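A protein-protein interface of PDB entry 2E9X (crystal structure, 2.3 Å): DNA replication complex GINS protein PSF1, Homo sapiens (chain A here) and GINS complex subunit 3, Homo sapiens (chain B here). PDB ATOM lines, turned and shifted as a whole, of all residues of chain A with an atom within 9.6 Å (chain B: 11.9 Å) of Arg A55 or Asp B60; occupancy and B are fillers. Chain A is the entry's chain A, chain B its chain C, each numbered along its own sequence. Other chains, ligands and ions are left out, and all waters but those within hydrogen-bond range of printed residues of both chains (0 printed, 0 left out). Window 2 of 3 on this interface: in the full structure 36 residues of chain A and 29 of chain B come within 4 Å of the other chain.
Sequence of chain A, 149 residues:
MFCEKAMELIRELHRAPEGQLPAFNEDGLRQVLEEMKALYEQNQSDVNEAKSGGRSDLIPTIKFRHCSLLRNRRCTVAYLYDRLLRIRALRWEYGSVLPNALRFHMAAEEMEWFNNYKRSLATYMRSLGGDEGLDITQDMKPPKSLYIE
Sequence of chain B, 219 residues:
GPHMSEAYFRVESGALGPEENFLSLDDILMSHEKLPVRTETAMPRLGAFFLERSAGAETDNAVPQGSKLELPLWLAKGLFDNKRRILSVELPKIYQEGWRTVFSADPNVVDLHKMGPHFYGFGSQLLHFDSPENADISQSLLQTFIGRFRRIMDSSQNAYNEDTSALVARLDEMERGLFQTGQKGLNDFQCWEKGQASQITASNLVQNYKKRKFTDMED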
ATOM      1  N   GLN A  42     -22.204   4.912  10.496  1.00  0.00           N
ATOM      2  CA  GLN A  42     -22.036   6.217  11.120  1.00  0.00           C
ATOM      3  C   GLN A  42     -20.570   6.494  11.406  1.00  0.00           C
ATOM      4  O   GLN A  42     -20.118   7.635  11.316  1.00  0.00           O
ATOM      5  CB  GLN A  42     -22.821   6.301  12.427  1.00  0.00           C
ATOM      6  CG  GLN A  42     -24.319   6.172  12.264  1.00  0.00           C
ATOM      7  CD  GLN A  42     -25.065   6.538  13.534  1.00  0.00           C
ATOM      8  OE1 GLN A  42     -25.002   7.682  13.994  1.00  0.00           O
ATOM      9  NE2 GLN A  42     -25.775   5.569  14.109  1.00  0.00           N
ATOM     10  N   SER A  45     -18.572   7.481   8.046  1.00  0.00           N
ATOM     11  CA  SER A  45     -18.707   8.873   7.649  1.00  0.00           C
ATOM     12  C   SER A  45     -17.958   9.803   8.604  1.00  0.00           C
ATOM     13  O   SER A  45     -17.295  10.747   8.171  1.00  0.00           O
ATOM     14  CB  SER A  45     -20.186   9.264   7.587  1.00  0.00           C
ATOM     15  OG  SER A  45     -20.817   9.082   8.840  1.00  0.00           O
ATOM     16  N   ASP A  46     -18.058   9.534   9.902  1.00  0.00           N
ATOM     17  CA  ASP A  46     -17.382  10.357  10.897  1.00  0.00           C
ATOM     18  C   ASP A  46     -15.870  10.254  10.759  1.00  0.00           C
ATOM     19  O   ASP A  46     -15.162  11.251  10.894  1.00  0.00           O
ATOM     20  CB  ASP A  46     -17.820   9.947  12.302  1.00  0.00           C
ATOM     21  CG  ASP A  46     -19.221  10.423  12.632  1.00  0.00           C
ATOM     22  OD1 ASP A  46     -20.093  10.363  11.739  1.00  0.00           O
ATOM     23  OD2 ASP A  46     -19.454  10.852  13.782  1.00  0.00           O
ATOM     24  N   VAL A  47     -15.377   9.052  10.484  1.00  0.00           N
ATOM     25  CA  VAL A  47     -13.943   8.851  10.309  1.00  0.00           C
ATOM     26  C   VAL A  47     -13.519   9.561   9.029  1.00  0.00           C
ATOM     27  O   VAL A  47     -12.337   9.829   8.810  1.00  0.00           O
ATOM     28  CB  VAL A  47     -13.589   7.345  10.205  1.00  0.00           C
ATOM     29  CG1 VAL A  47     -12.130   7.168   9.820  1.00  0.00           C
ATOM     30  CG2 VAL A  47     -13.847   6.664  11.534  1.00  0.00           C
ATOM     31  N   ASN A  48     -14.500   9.870   8.188  1.00  0.00           N
ATOM     32  CA  ASN A  48     -14.231  10.558   6.936  1.00  0.00           C
ATOM     33  C   ASN A  48     -14.194  12.059   7.205  1.00  0.00           C
ATOM     34  O   ASN A  48     -13.354  12.770   6.656  1.00  0.00           O
ATOM     35  CB  ASN A  48     -15.310  10.226   5.904  1.00  0.00           C
ATOM     36  CG  ASN A  48     -14.909  10.621   4.498  1.00  0.00           C
ATOM     37  OD1 ASN A  48     -14.716  11.802   4.201  1.00  0.00           O
ATOM     38  ND2 ASN A  48     -14.775   9.630   3.621  1.00  0.00           N
ATOM     39  N   GLU A  49     -15.102  12.537   8.052  1.00  0.00           N
ATOM     40  CA  GLU A  49     -15.132  13.953   8.402  1.00  0.00           C
ATOM     41  C   GLU A  49     -13.876  14.294   9.190  1.00  0.00           C
ATOM     42  O   GLU A  49     -13.453  15.449   9.236  1.00  0.00           O
ATOM     43  CB  GLU A  49     -16.358  14.288   9.251  1.00  0.00           C
ATOM     44  CG  GLU A  49     -17.649  14.438   8.478  1.00  0.00           C
ATOM     45  CD  GLU A  49     -18.745  15.066   9.318  1.00  0.00           C
ATOM     46  OE1 GLU A  49     -18.529  16.184   9.836  1.00  0.00           O
ATOM     47  OE2 GLU A  49     -19.822  14.449   9.464  1.00  0.00           O
ATOM     48  N   ALA A  50     -13.289  13.279   9.818  1.00  0.00           N
ATOM     49  CA  ALA A  50     -12.074  13.458  10.602  1.00  0.00           C
ATOM     50  C   ALA A  50     -10.857  13.273   9.701  1.00  0.00           C
ATOM     51  O   ALA A  50      -9.714  13.384  10.148  1.00  0.00           O
ATOM     52  CB  ALA A  50     -12.038  12.456  11.746  1.00  0.00           C
ATOM     53  N   LYS A  51     -11.116  12.986   8.430  1.00  0.00           N
ATOM     54  CA  LYS A  51     -10.059  12.783   7.445  1.00  0.00           C
ATOM     55  C   LYS A  51     -10.137  13.868   6.375  1.00  0.00           C
ATOM     56  O   LYS A  51      -9.175  14.103   5.642  1.00  0.00           O
ATOM     57  CB  LYS A  51     -10.204  11.403   6.795  1.00  0.00           C
ATOM     58  CG  LYS A  51      -9.188  11.102   5.700  1.00  0.00           C
ATOM     59  CD  LYS A  51      -7.770  11.013   6.246  1.00  0.00           C
ATOM     60  CE  LYS A  51      -6.787  10.624   5.147  1.00  0.00           C
ATOM     61  NZ  LYS A  51      -5.386  10.509   5.645  1.00  0.00           N
ATOM     62  N   SER A  52     -11.290  14.526   6.294  1.00  0.00           N
ATOM     63  CA  SER A  52     -11.511  15.586   5.319  1.00  0.00           C
ATOM     64  C   SER A  52     -12.344  16.702   5.935  1.00  0.00           C
ATOM     65  O   SER A  52     -13.436  17.013   5.455  1.00  0.00           O
ATOM     66  CB  SER A  52     -12.229  15.028   4.089  1.00  0.00           C
ATOM     67  OG  SER A  52     -11.478  13.987   3.492  1.00  0.00           O
ATOM     68  N   GLY A  53     -11.823  17.296   7.004  1.00  0.00           N
ATOM     69  CA  GLY A  53     -12.529  18.371   7.676  1.00  0.00           C
ATOM     70  C   GLY A  53     -11.869  18.728   8.993  1.00  0.00           C
ATOM     71  O   GLY A  53     -12.349  19.599   9.722  1.00  0.00           O
ATOM     72  N   GLY A  54     -10.765  18.051   9.299  1.00  0.00           N
ATOM     73  CA  GLY A  54     -10.052  18.309  10.537  1.00  0.00           C
ATOM     74  C   GLY A  54     -10.937  18.151  11.757  1.00  0.00           C
ATOM     75  O   GLY A  54     -10.891  18.967  12.680  1.00  0.00           O
ATOM     76  N   ARG A  55     -11.749  17.099  11.762  1.00  0.00           N
ATOM     77  CA  ARG A  55     -12.652  16.840  12.877  1.00  0.00           C
ATOM     78  C   ARG A  55     -12.103  15.783  13.829  1.00  0.00           C
ATOM     79  O   ARG A  55     -12.760  14.773  14.091  1.00  0.00           O
ATOM     80  CB  ARG A  55     -14.025  16.397  12.357  1.00  0.00           C
ATOM     81  CG  ARG A  55     -14.760  17.453  11.551  1.00  0.00           C
ATOM     82  CD  ARG A  55     -14.957  18.728  12.358  1.00  0.00           C
ATOM     83  NE  ARG A  55     -15.816  18.549  13.527  1.00  0.00           N
ATOM     84  CZ  ARG A  55     -17.100  18.208  13.471  1.00  0.00           C
ATOM     85  NH1 ARG A  55     -17.683  18.000  12.300  1.00  0.00           N
ATOM     86  NH2 ARG A  55     -17.808  18.094  14.586  1.00  0.00           N
ATOM     87  N   SER A  56     -10.900  16.013  14.347  1.00  0.00           N
ATOM     88  CA  SER A  56     -10.294  15.070  15.279  1.00  0.00           C
ATOM     89  C   SER A  56     -11.100  15.082  16.576  1.00  0.00           C
ATOM     90  O   SER A  56     -10.866  14.275  17.477  1.00  0.00           O
ATOM     91  CB  SER A  56      -8.837  15.452  15.561  1.00  0.00           C
ATOM     92  OG  SER A  56      -8.746  16.715  16.194  1.00  0.00           O
ATOM     93  N   ASP A  57     -12.055  16.005  16.656  1.00  0.00           N
ATOM     94  CA  ASP A  57     -12.919  16.138  17.823  1.00  0.00           C
ATOM     95  C   ASP A  57     -14.037  15.097  17.762  1.00  0.00           C
ATOM     96  O   ASP A  57     -14.920  15.059  18.623  1.00  0.00           O
ATOM     97  CB  ASP A  57     -13.523  17.543  17.869  1.00  0.00           C
ATOM     98  CG  ASP A  57     -14.405  17.838  16.667  1.00  0.00           C
ATOM     99  OD1 ASP A  57     -13.941  17.626  15.526  1.00  0.00           O
ATOM    100  OD2 ASP A  57     -15.556  18.286  16.864  1.00  0.00           O
ATOM    101  N   LEU A  58     -13.995  14.263  16.728  1.00  0.00           N
ATOM    102  CA  LEU A  58     -14.991  13.217  16.543  1.00  0.00           C
ATOM    103  C   LEU A  58     -14.441  11.868  16.985  1.00  0.00           C
ATOM    104  O   LEU A  58     -15.188  10.905  17.121  1.00  0.00           O
ATOM    105  CB  LEU A  58     -15.419  13.133  15.073  1.00  0.00           C
ATOM    106  CG  LEU A  58     -16.247  14.291  14.512  1.00  0.00           C
ATOM    107  CD1 LEU A  58     -16.560  14.028  13.047  1.00  0.00           C
ATOM    108  CD2 LEU A  58     -17.533  14.445  15.311  1.00  0.00           C
ATOM    109  N   ILE A  59     -13.132  11.804  17.207  1.00  0.00           N
ATOM    110  CA  ILE A  59     -12.493  10.566  17.632  1.00  0.00           C
ATOM    111  C   ILE A  59     -13.158   9.947  18.863  1.00  0.00           C
ATOM    112  O   ILE A  59     -13.377   8.739  18.908  1.00  0.00           O
ATOM    113  CB  ILE A  59     -10.984  10.780  17.902  1.00  0.00           C
ATOM    114  CG1 ILE A  59     -10.231  10.808  16.569  1.00  0.00           C
ATOM    115  CG2 ILE A  59     -10.444   9.684  18.813  1.00  0.00           C
ATOM    116  CD1 ILE A  59      -8.722  10.906  16.701  1.00  0.00           C
ATOM    117  N   PRO A  60     -13.483  10.766  19.878  1.00  0.00           N
ATOM    118  CA  PRO A  60     -14.125  10.221  21.079  1.00  0.00           C
ATOM    119  C   PRO A  60     -15.407   9.477  20.718  1.00  0.00           C
ATOM    120  O   PRO A  60     -15.664   8.380  21.211  1.00  0.00           O
ATOM    121  CB  PRO A  60     -14.398  11.468  21.917  1.00  0.00           C
ATOM    122  CG  PRO A  60     -13.257  12.369  21.545  1.00  0.00           C
ATOM    123  CD  PRO A  60     -13.204  12.205  20.042  1.00  0.00           C
ATOM    124  N   THR A  61     -16.208  10.089  19.853  1.00  0.00           N
ATOM    125  CA  THR A  61     -17.459   9.491  19.415  1.00  0.00           C
ATOM    126  C   THR A  61     -17.163   8.266  18.562  1.00  0.00           C
ATOM    127  O   THR A  61     -17.922   7.296  18.564  1.00  0.00           O
ATOM    128  CB  THR A  61     -18.288  10.486  18.585  1.00  0.00           C
ATOM    129  OG1 THR A  61     -18.589  11.638  19.386  1.00  0.00           O
ATOM    130  CG2 THR A  61     -19.592   9.841  18.116  1.00  0.00           C
ATOM    131  N   ILE A  62     -16.051   8.316  17.837  1.00  0.00           N
ATOM    132  CA  ILE A  62     -15.657   7.212  16.977  1.00  0.00           C
ATOM    133  C   ILE A  62     -15.300   5.978  17.802  1.00  0.00           C
ATOM    134  O   ILE A  62     -15.798   4.887  17.526  1.00  0.00           O
ATOM    135  CB  ILE A  62     -14.463   7.605  16.070  1.00  0.00           C
ATOM    136  CG1 ILE A  62     -14.904   8.686  15.076  1.00  0.00           C
ATOM    137  CG2 ILE A  62     -13.943   6.388  15.321  1.00  0.00           C
ATOM    138  CD1 ILE A  62     -13.811   9.123  14.105  1.00  0.00           C
ATOM    139  N   ARG A  65     -18.410   4.356  19.330  1.00  0.00           N
ATOM    140  CA  ARG A  65     -19.152   3.449  18.470  1.00  0.00           C
ATOM    141  C   ARG A  65     -18.364   2.166  18.262  1.00  0.00           C
ATOM    142  O   ARG A  65     -18.937   1.085  18.136  1.00  0.00           O
ATOM    143  CB  ARG A  65     -19.442   4.098  17.115  1.00  0.00           C
ATOM    144  CG  ARG A  65     -20.311   5.346  17.184  1.00  0.00           C
ATOM    145  CD  ARG A  65     -21.061   5.547  15.873  1.00  0.00           C
ATOM    146  NE  ARG A  65     -21.633   6.886  15.749  1.00  0.00           N
ATOM    147  CZ  ARG A  65     -20.928   7.982  15.472  1.00  0.00           C
ATOM    148  NH1 ARG A  65     -19.614   7.902  15.287  1.00  0.00           N
ATOM    149  NH2 ARG A  65     -21.539   9.156  15.369  1.00  0.00           N
ATOM    150  N   THR B  41     -13.712  15.376  27.678  1.00  0.00           N
ATOM    151  CA  THR B  41     -13.803  15.957  26.344  1.00  0.00           C
ATOM    152  C   THR B  41     -15.245  15.828  25.879  1.00  0.00           C
ATOM    153  O   THR B  41     -15.985  14.965  26.355  1.00  0.00           O
ATOM    154  CB  THR B  41     -12.907  15.210  25.337  1.00  0.00           C
ATOM    155  OG1 THR B  41     -11.543  15.271  25.771  1.00  0.00           O
ATOM    156  CG2 THR B  41     -13.020  15.836  23.954  1.00  0.00           C
ATOM    157  N   ALA B  42     -15.650  16.689  24.955  1.00  0.00           N
ATOM    158  CA  ALA B  42     -17.008  16.631  24.443  1.00  0.00           C
ATOM    159  C   ALA B  42     -17.110  15.454  23.485  1.00  0.00           C
ATOM    160  O   ALA B  42     -16.122  15.056  22.866  1.00  0.00           O
ATOM    161  CB  ALA B  42     -17.355  17.922  23.728  1.00  0.00           C
ATOM    162  N   MET B  43     -18.308  14.894  23.380  1.00  0.00           N
ATOM    163  CA  MET B  43     -18.544  13.771  22.485  1.00  0.00           C
ATOM    164  C   MET B  43     -19.696  14.126  21.553  1.00  0.00           C
ATOM    165  O   MET B  43     -20.866  13.981  21.904  1.00  0.00           O
ATOM    166  CB  MET B  43     -18.867  12.509  23.287  1.00  0.00           C
ATOM    167  CG  MET B  43     -17.722  12.054  24.176  1.00  0.00           C
ATOM    168  SD  MET B  43     -18.021  10.458  24.966  1.00  0.00           S
ATOM    169  CE  MET B  43     -17.312   9.350  23.758  1.00  0.00           C
ATOM    170  N   PRO B  44     -19.365  14.609  20.346  1.00  0.00           N
ATOM    171  CA  PRO B  44     -20.330  15.011  19.321  1.00  0.00           C
ATOM    172  C   PRO B  44     -21.337  13.939  18.922  1.00  0.00           C
ATOM    173  O   PRO B  44     -20.997  12.764  18.796  1.00  0.00           O
ATOM    174  CB  PRO B  44     -19.438  15.413  18.148  1.00  0.00           C
ATOM    175  CG  PRO B  44     -18.188  15.892  18.819  1.00  0.00           C
ATOM    176  CD  PRO B  44     -17.986  14.845  19.880  1.00  0.00           C
ATOM    177  N   ARG B  45     -22.583  14.361  18.737  1.00  0.00           N
ATOM    178  CA  ARG B  45     -23.645  13.465  18.299  1.00  0.00           C
ATOM    179  C   ARG B  45     -23.921  12.270  19.213  1.00  0.00           C
ATOM    180  O   ARG B  45     -24.127  11.157  18.733  1.00  0.00           O
ATOM    181  CB  ARG B  45     -23.310  12.977  16.887  1.00  0.00           C
ATOM    182  CG  ARG B  45     -23.008  14.125  15.938  1.00  0.00           C
ATOM    183  CD  ARG B  45     -22.033  13.738  14.842  1.00  0.00           C
ATOM    184  NE  ARG B  45     -21.647  14.902  14.045  1.00  0.00           N
ATOM    185  CZ  ARG B  45     -20.726  14.884  13.086  1.00  0.00           C
ATOM    186  NH1 ARG B  45     -20.085  13.761  12.799  1.00  0.00           N
ATOM    187  NH2 ARG B  45     -20.445  15.996  12.417  1.00  0.00           N
ATOM    188  N   LEU B  46     -23.937  12.504  20.522  1.00  0.00           N
ATOM    189  CA  LEU B  46     -24.199  11.432  21.480  1.00  0.00           C
ATOM    190  C   LEU B  46     -25.079  11.890  22.639  1.00  0.00           C
ATOM    191  O   LEU B  46     -25.560  11.068  23.421  1.00  0.00           O
ATOM    192  CB  LEU B  46     -22.883  10.877  22.035  1.00  0.00           C
ATOM    193  CG  LEU B  46     -21.955  10.147  21.063  1.00  0.00           C
ATOM    194  CD1 LEU B  46     -20.709   9.691  21.806  1.00  0.00           C
ATOM    195  CD2 LEU B  46     -22.676   8.955  20.450  1.00  0.00           C
ATOM    196  N   GLY B  47     -25.286  13.199  22.747  1.00  0.00           N
ATOM    197  CA  GLY B  47     -26.104  13.733  23.822  1.00  0.00           C
ATOM    198  C   GLY B  47     -27.493  13.128  23.880  1.00  0.00           C
ATOM    199  O   GLY B  47     -28.151  13.162  24.922  1.00  0.00           O
ATOM    200  N   ALA B  48     -27.939  12.569  22.759  1.00  0.00           N
ATOM    201  CA  ALA B  48     -29.261  11.956  22.671  1.00  0.00           C
ATOM    202  C   ALA B  48     -29.421  10.794  23.650  1.00  0.00           C
ATOM    203  O   ALA B  48     -30.536  10.469  24.063  1.00  0.00           O
ATOM    204  CB  ALA B  48     -29.514  11.475  21.247  1.00  0.00           C
ATOM    205  N   PHE B  49     -28.306  10.173  24.019  1.00  0.00           N
ATOM    206  CA  PHE B  49     -28.331   9.049  24.945  1.00  0.00           C
ATOM    207  C   PHE B  49     -28.214   9.489  26.399  1.00  0.00           C
ATOM    208  O   PHE B  49     -28.347   8.676  27.313  1.00  0.00           O
ATOM    209  CB  PHE B  49     -27.200   8.070  24.620  1.00  0.00           C
ATOM    210  CG  PHE B  49     -27.260   7.513  23.226  1.00  0.00           C
ATOM    211  CD1 PHE B  49     -28.459   7.038  22.702  1.00  0.00           C
ATOM    212  CD2 PHE B  49     -26.112   7.439  22.445  1.00  0.00           C
ATOM    213  CE1 PHE B  49     -28.514   6.497  21.424  1.00  0.00           C
ATOM    214  CE2 PHE B  49     -26.157   6.902  21.165  1.00  0.00           C
ATOM    215  CZ  PHE B  49     -27.360   6.430  20.654  1.00  0.00           C
ATOM    216  N   PHE B  50     -27.963  10.777  26.611  1.00  0.00           N
ATOM    217  CA  PHE B  50     -27.824  11.307  27.963  1.00  0.00           C
ATOM    218  C   PHE B  50     -28.489  12.677  28.088  1.00  0.00           C
ATOM    219  O   PHE B  50     -29.586  12.802  28.635  1.00  0.00           O
ATOM    220  CB  PHE B  50     -26.342  11.418  28.339  1.00  0.00           C
ATOM    221  CG  PHE B  50     -25.513  10.230  27.919  1.00  0.00           C
ATOM    222  CD1 PHE B  50     -25.053  10.112  26.611  1.00  0.00           C
ATOM    223  CD2 PHE B  50     -25.198   9.226  28.831  1.00  0.00           C
ATOM    224  CE1 PHE B  50     -24.291   9.014  26.216  1.00  0.00           C
ATOM    225  CE2 PHE B  50     -24.436   8.122  28.444  1.00  0.00           C
ATOM    226  CZ  PHE B  50     -23.982   8.017  27.134  1.00  0.00           C
ATOM    227  N   ASP B  60     -23.073  19.801  17.631  1.00  0.00           N
ATOM    228  CA  ASP B  60     -23.370  18.550  16.945  1.00  0.00           C
ATOM    229  C   ASP B  60     -24.225  17.630  17.811  1.00  0.00           C
ATOM    230  O   ASP B  60     -24.103  16.410  17.728  1.00  0.00           O
ATOM    231  CB  ASP B  60     -22.070  17.825  16.574  1.00  0.00           C
ATOM    232  CG  ASP B  60     -21.261  18.570  15.528  1.00  0.00           C
ATOM    233  OD1 ASP B  60     -21.776  18.769  14.408  1.00  0.00           O
ATOM    234  OD2 ASP B  60     -20.109  18.953  15.824  1.00  0.00           O
ATOM    235  N   ASN B  61     -25.093  18.211  18.638  1.00  0.00           N
ATOM    236  CA  ASN B  61     -25.948  17.414  19.513  1.00  0.00           C
ATOM    237  C   ASN B  61     -25.007  16.611  20.415  1.00  0.00           C
ATOM    238  O   ASN B  61     -25.339  15.524  20.890  1.00  0.00           O
ATOM    239  CB  ASN B  61     -26.815  16.473  18.664  1.00  0.00           C
ATOM    240  CG  ASN B  61     -27.942  15.836  19.453  1.00  0.00           C
ATOM    241  OD1 ASN B  61     -27.712  15.132  20.437  1.00  0.00           O
ATOM    242  ND2 ASN B  61     -29.174  16.077  19.017  1.00  0.00           N
ATOM    243  N   ALA B  62     -23.826  17.178  20.641  1.00  0.00           N
ATOM    244  CA  ALA B  62     -22.782  16.556  21.443  1.00  0.00           C
ATOM    245  C   ALA B  62     -23.063  16.467  22.937  1.00  0.00           C
ATOM    246  O   ALA B  62     -24.060  16.990  23.437  1.00  0.00           O
ATOM    247  CB  ALA B  62     -21.469  17.294  21.221  1.00  0.00           C
ATOM    248  N   VAL B  63     -22.156  15.788  23.635  1.00  0.00           N
ATOM    249  CA  VAL B  63     -22.231  15.610  25.079  1.00  0.00           C
ATOM    250  C   VAL B  63     -21.167  16.514  25.687  1.00  0.00           C
ATOM    251  O   VAL B  63     -19.972  16.326  25.452  1.00  0.00           O
ATOM    252  CB  VAL B  63     -21.934  14.148  25.490  1.00  0.00           C
ATOM    253  CG1 VAL B  63     -21.988  14.014  27.004  1.00  0.00           C
ATOM    254  CG2 VAL B  63     -22.934  13.207  24.841  1.00  0.00           C
ATOM    255  N   PRO B  64     -21.589  17.511  26.476  1.00  0.00           N
ATOM    256  CA  PRO B  64     -20.667  18.452  27.119  1.00  0.00           C
ATOM    257  C   PRO B  64     -19.524  17.736  27.822  1.00  0.00           C
ATOM    258  O   PRO B  64     -19.672  16.587  28.241  1.00  0.00           O
ATOM    259  CB  PRO B  64     -21.566  19.189  28.108  1.00  0.00           C
ATOM    260  CG  PRO B  64     -22.895  19.176  27.425  1.00  0.00           C
ATOM    261  CD  PRO B  64     -22.975  17.762  26.907  1.00  0.00           C
ATOM    262  N   GLN B  65     -18.382  18.406  27.943  1.00  0.00           N
ATOM    263  CA  GLN B  65     -17.250  17.806  28.635  1.00  0.00           C
ATOM    264  C   GLN B  65     -17.509  18.004  30.125  1.00  0.00           C
ATOM    265  O   GLN B  65     -18.311  18.859  30.511  1.00  0.00           O
ATOM    266  CB  GLN B  65     -15.937  18.490  28.251  1.00  0.00           C
ATOM    267  CG  GLN B  65     -15.730  19.853  28.898  1.00  0.00           C
ATOM    268  CD  GLN B  65     -14.279  20.293  28.876  1.00  0.00           C
ATOM    269  OE1 GLN B  65     -13.403  19.608  29.409  1.00  0.00           O
ATOM    270  NE2 GLN B  65     -14.015  21.444  28.263  1.00  0.00           N
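The side-chain hydroxyl of Ser A45 lies within hydrogen-bond range of the side-chain carboxylate of Asp A46, at 3.3 Å. OD2 of Asp A46 lies within salt-bridge range of NH2 of Arg A65 (3.1 Å). NH1 of Arg A55 is in salt-bridge range of OE1 of Glu A49 (3.2 Å). The guanidinium group of Arg A55 lies within salt-bridge range of the side-chain carboxylate of Asp A57, at 2.9 Å. The backbone carbonyl oxygen (O) of Met B43 lies within hydrogen-bond range of the backbone NH (N) of Val B63. The side-chain carboxylate (OD1) of Asp B60 lies within salt-bridge range of the guanidinium group (NH2) of Arg B45 (3.7 Å).
The side-chain carboxylate (OD2) of Asp A46 lies within salt-bridge range of the guanidinium group (NH1) of Arg B45 (3.1 Å). The side-chain carboxylate (OE1) of Glu A49 is in salt-bridge range of the guanidinium group (NH2) of Arg B45. The side-chain carboxylate (OD2) of Asp B60 is in salt-bridge range of the guanidinium group (NH2) of Arg A55 (2.8 Å). The backbone carbonyl oxygen (O) of Pro B44 lies within hydrogen-bond range of the side-chain hydroxyl (OG1) of Thr A61. The guanidinium group (NH1) of Arg A55 sits close to the guanidinium group (NH2) of Arg B45.
Among the printed residues, pairs that only touch across the chains: Asp A57 with Pro B44, Leu A58 with Pro B44, Leu A58 with Arg B45, Pro A60 with Met B43, Thr A61 with Met B43 and Thr A61 with Leu B46.
Printed residues of chain B that touch a printed residue of chain A: Met B43, Pro B44, Arg B45, Leu B46 and Asp B60. Of the 20 printed residues of chain A, 7 touch a printed residue of chain B. Among the printed residues, 11 pairs touch across the chains. Among the printed residues, Asp or Glu carboxylates within 4 Å of a Lys or Arg side-chain nitrogen of the other chain: Asp A46 with Arg B45 (3.1 Å), Glu A49 with Arg B45 (3.2 Å) and Arg A55 with Asp B60 (2.8 Å).
Of the printed residues of chain B, Asp A46 touches Arg B45 (3.1 Å). Val A47 touches none of the printed residues of chain B. Glu A49 touches one residue of chain B. No residue of chain B comes within 4 Å of Ala A50. Ser A52 touches none of the printed residues of chain B. No residue of chain B comes within 4 Å of Gly A53. Arg A55 touches just these residues of chain B: Arg B45 and Asp B60. Asp A57 touches just one residue of chain B: Pro B44 (3.3 Å). No residue of chain B comes within 4 Å of Ile A59. Of the printed residues of chain B, Pro A60 touches Met B43 (3.2 Å). Arg B45 touches four residues of chain A. Of the printed residues of chain A, Leu B46 touches Thr A61. Printed residues of chain A within 4 Å of Asp B60: Arg A55. Asn B61 touches none of the printed residues of chain A. The nearest printed residue of chain A that does not touch Pro B44 is Arg A55 (4.7 Å).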
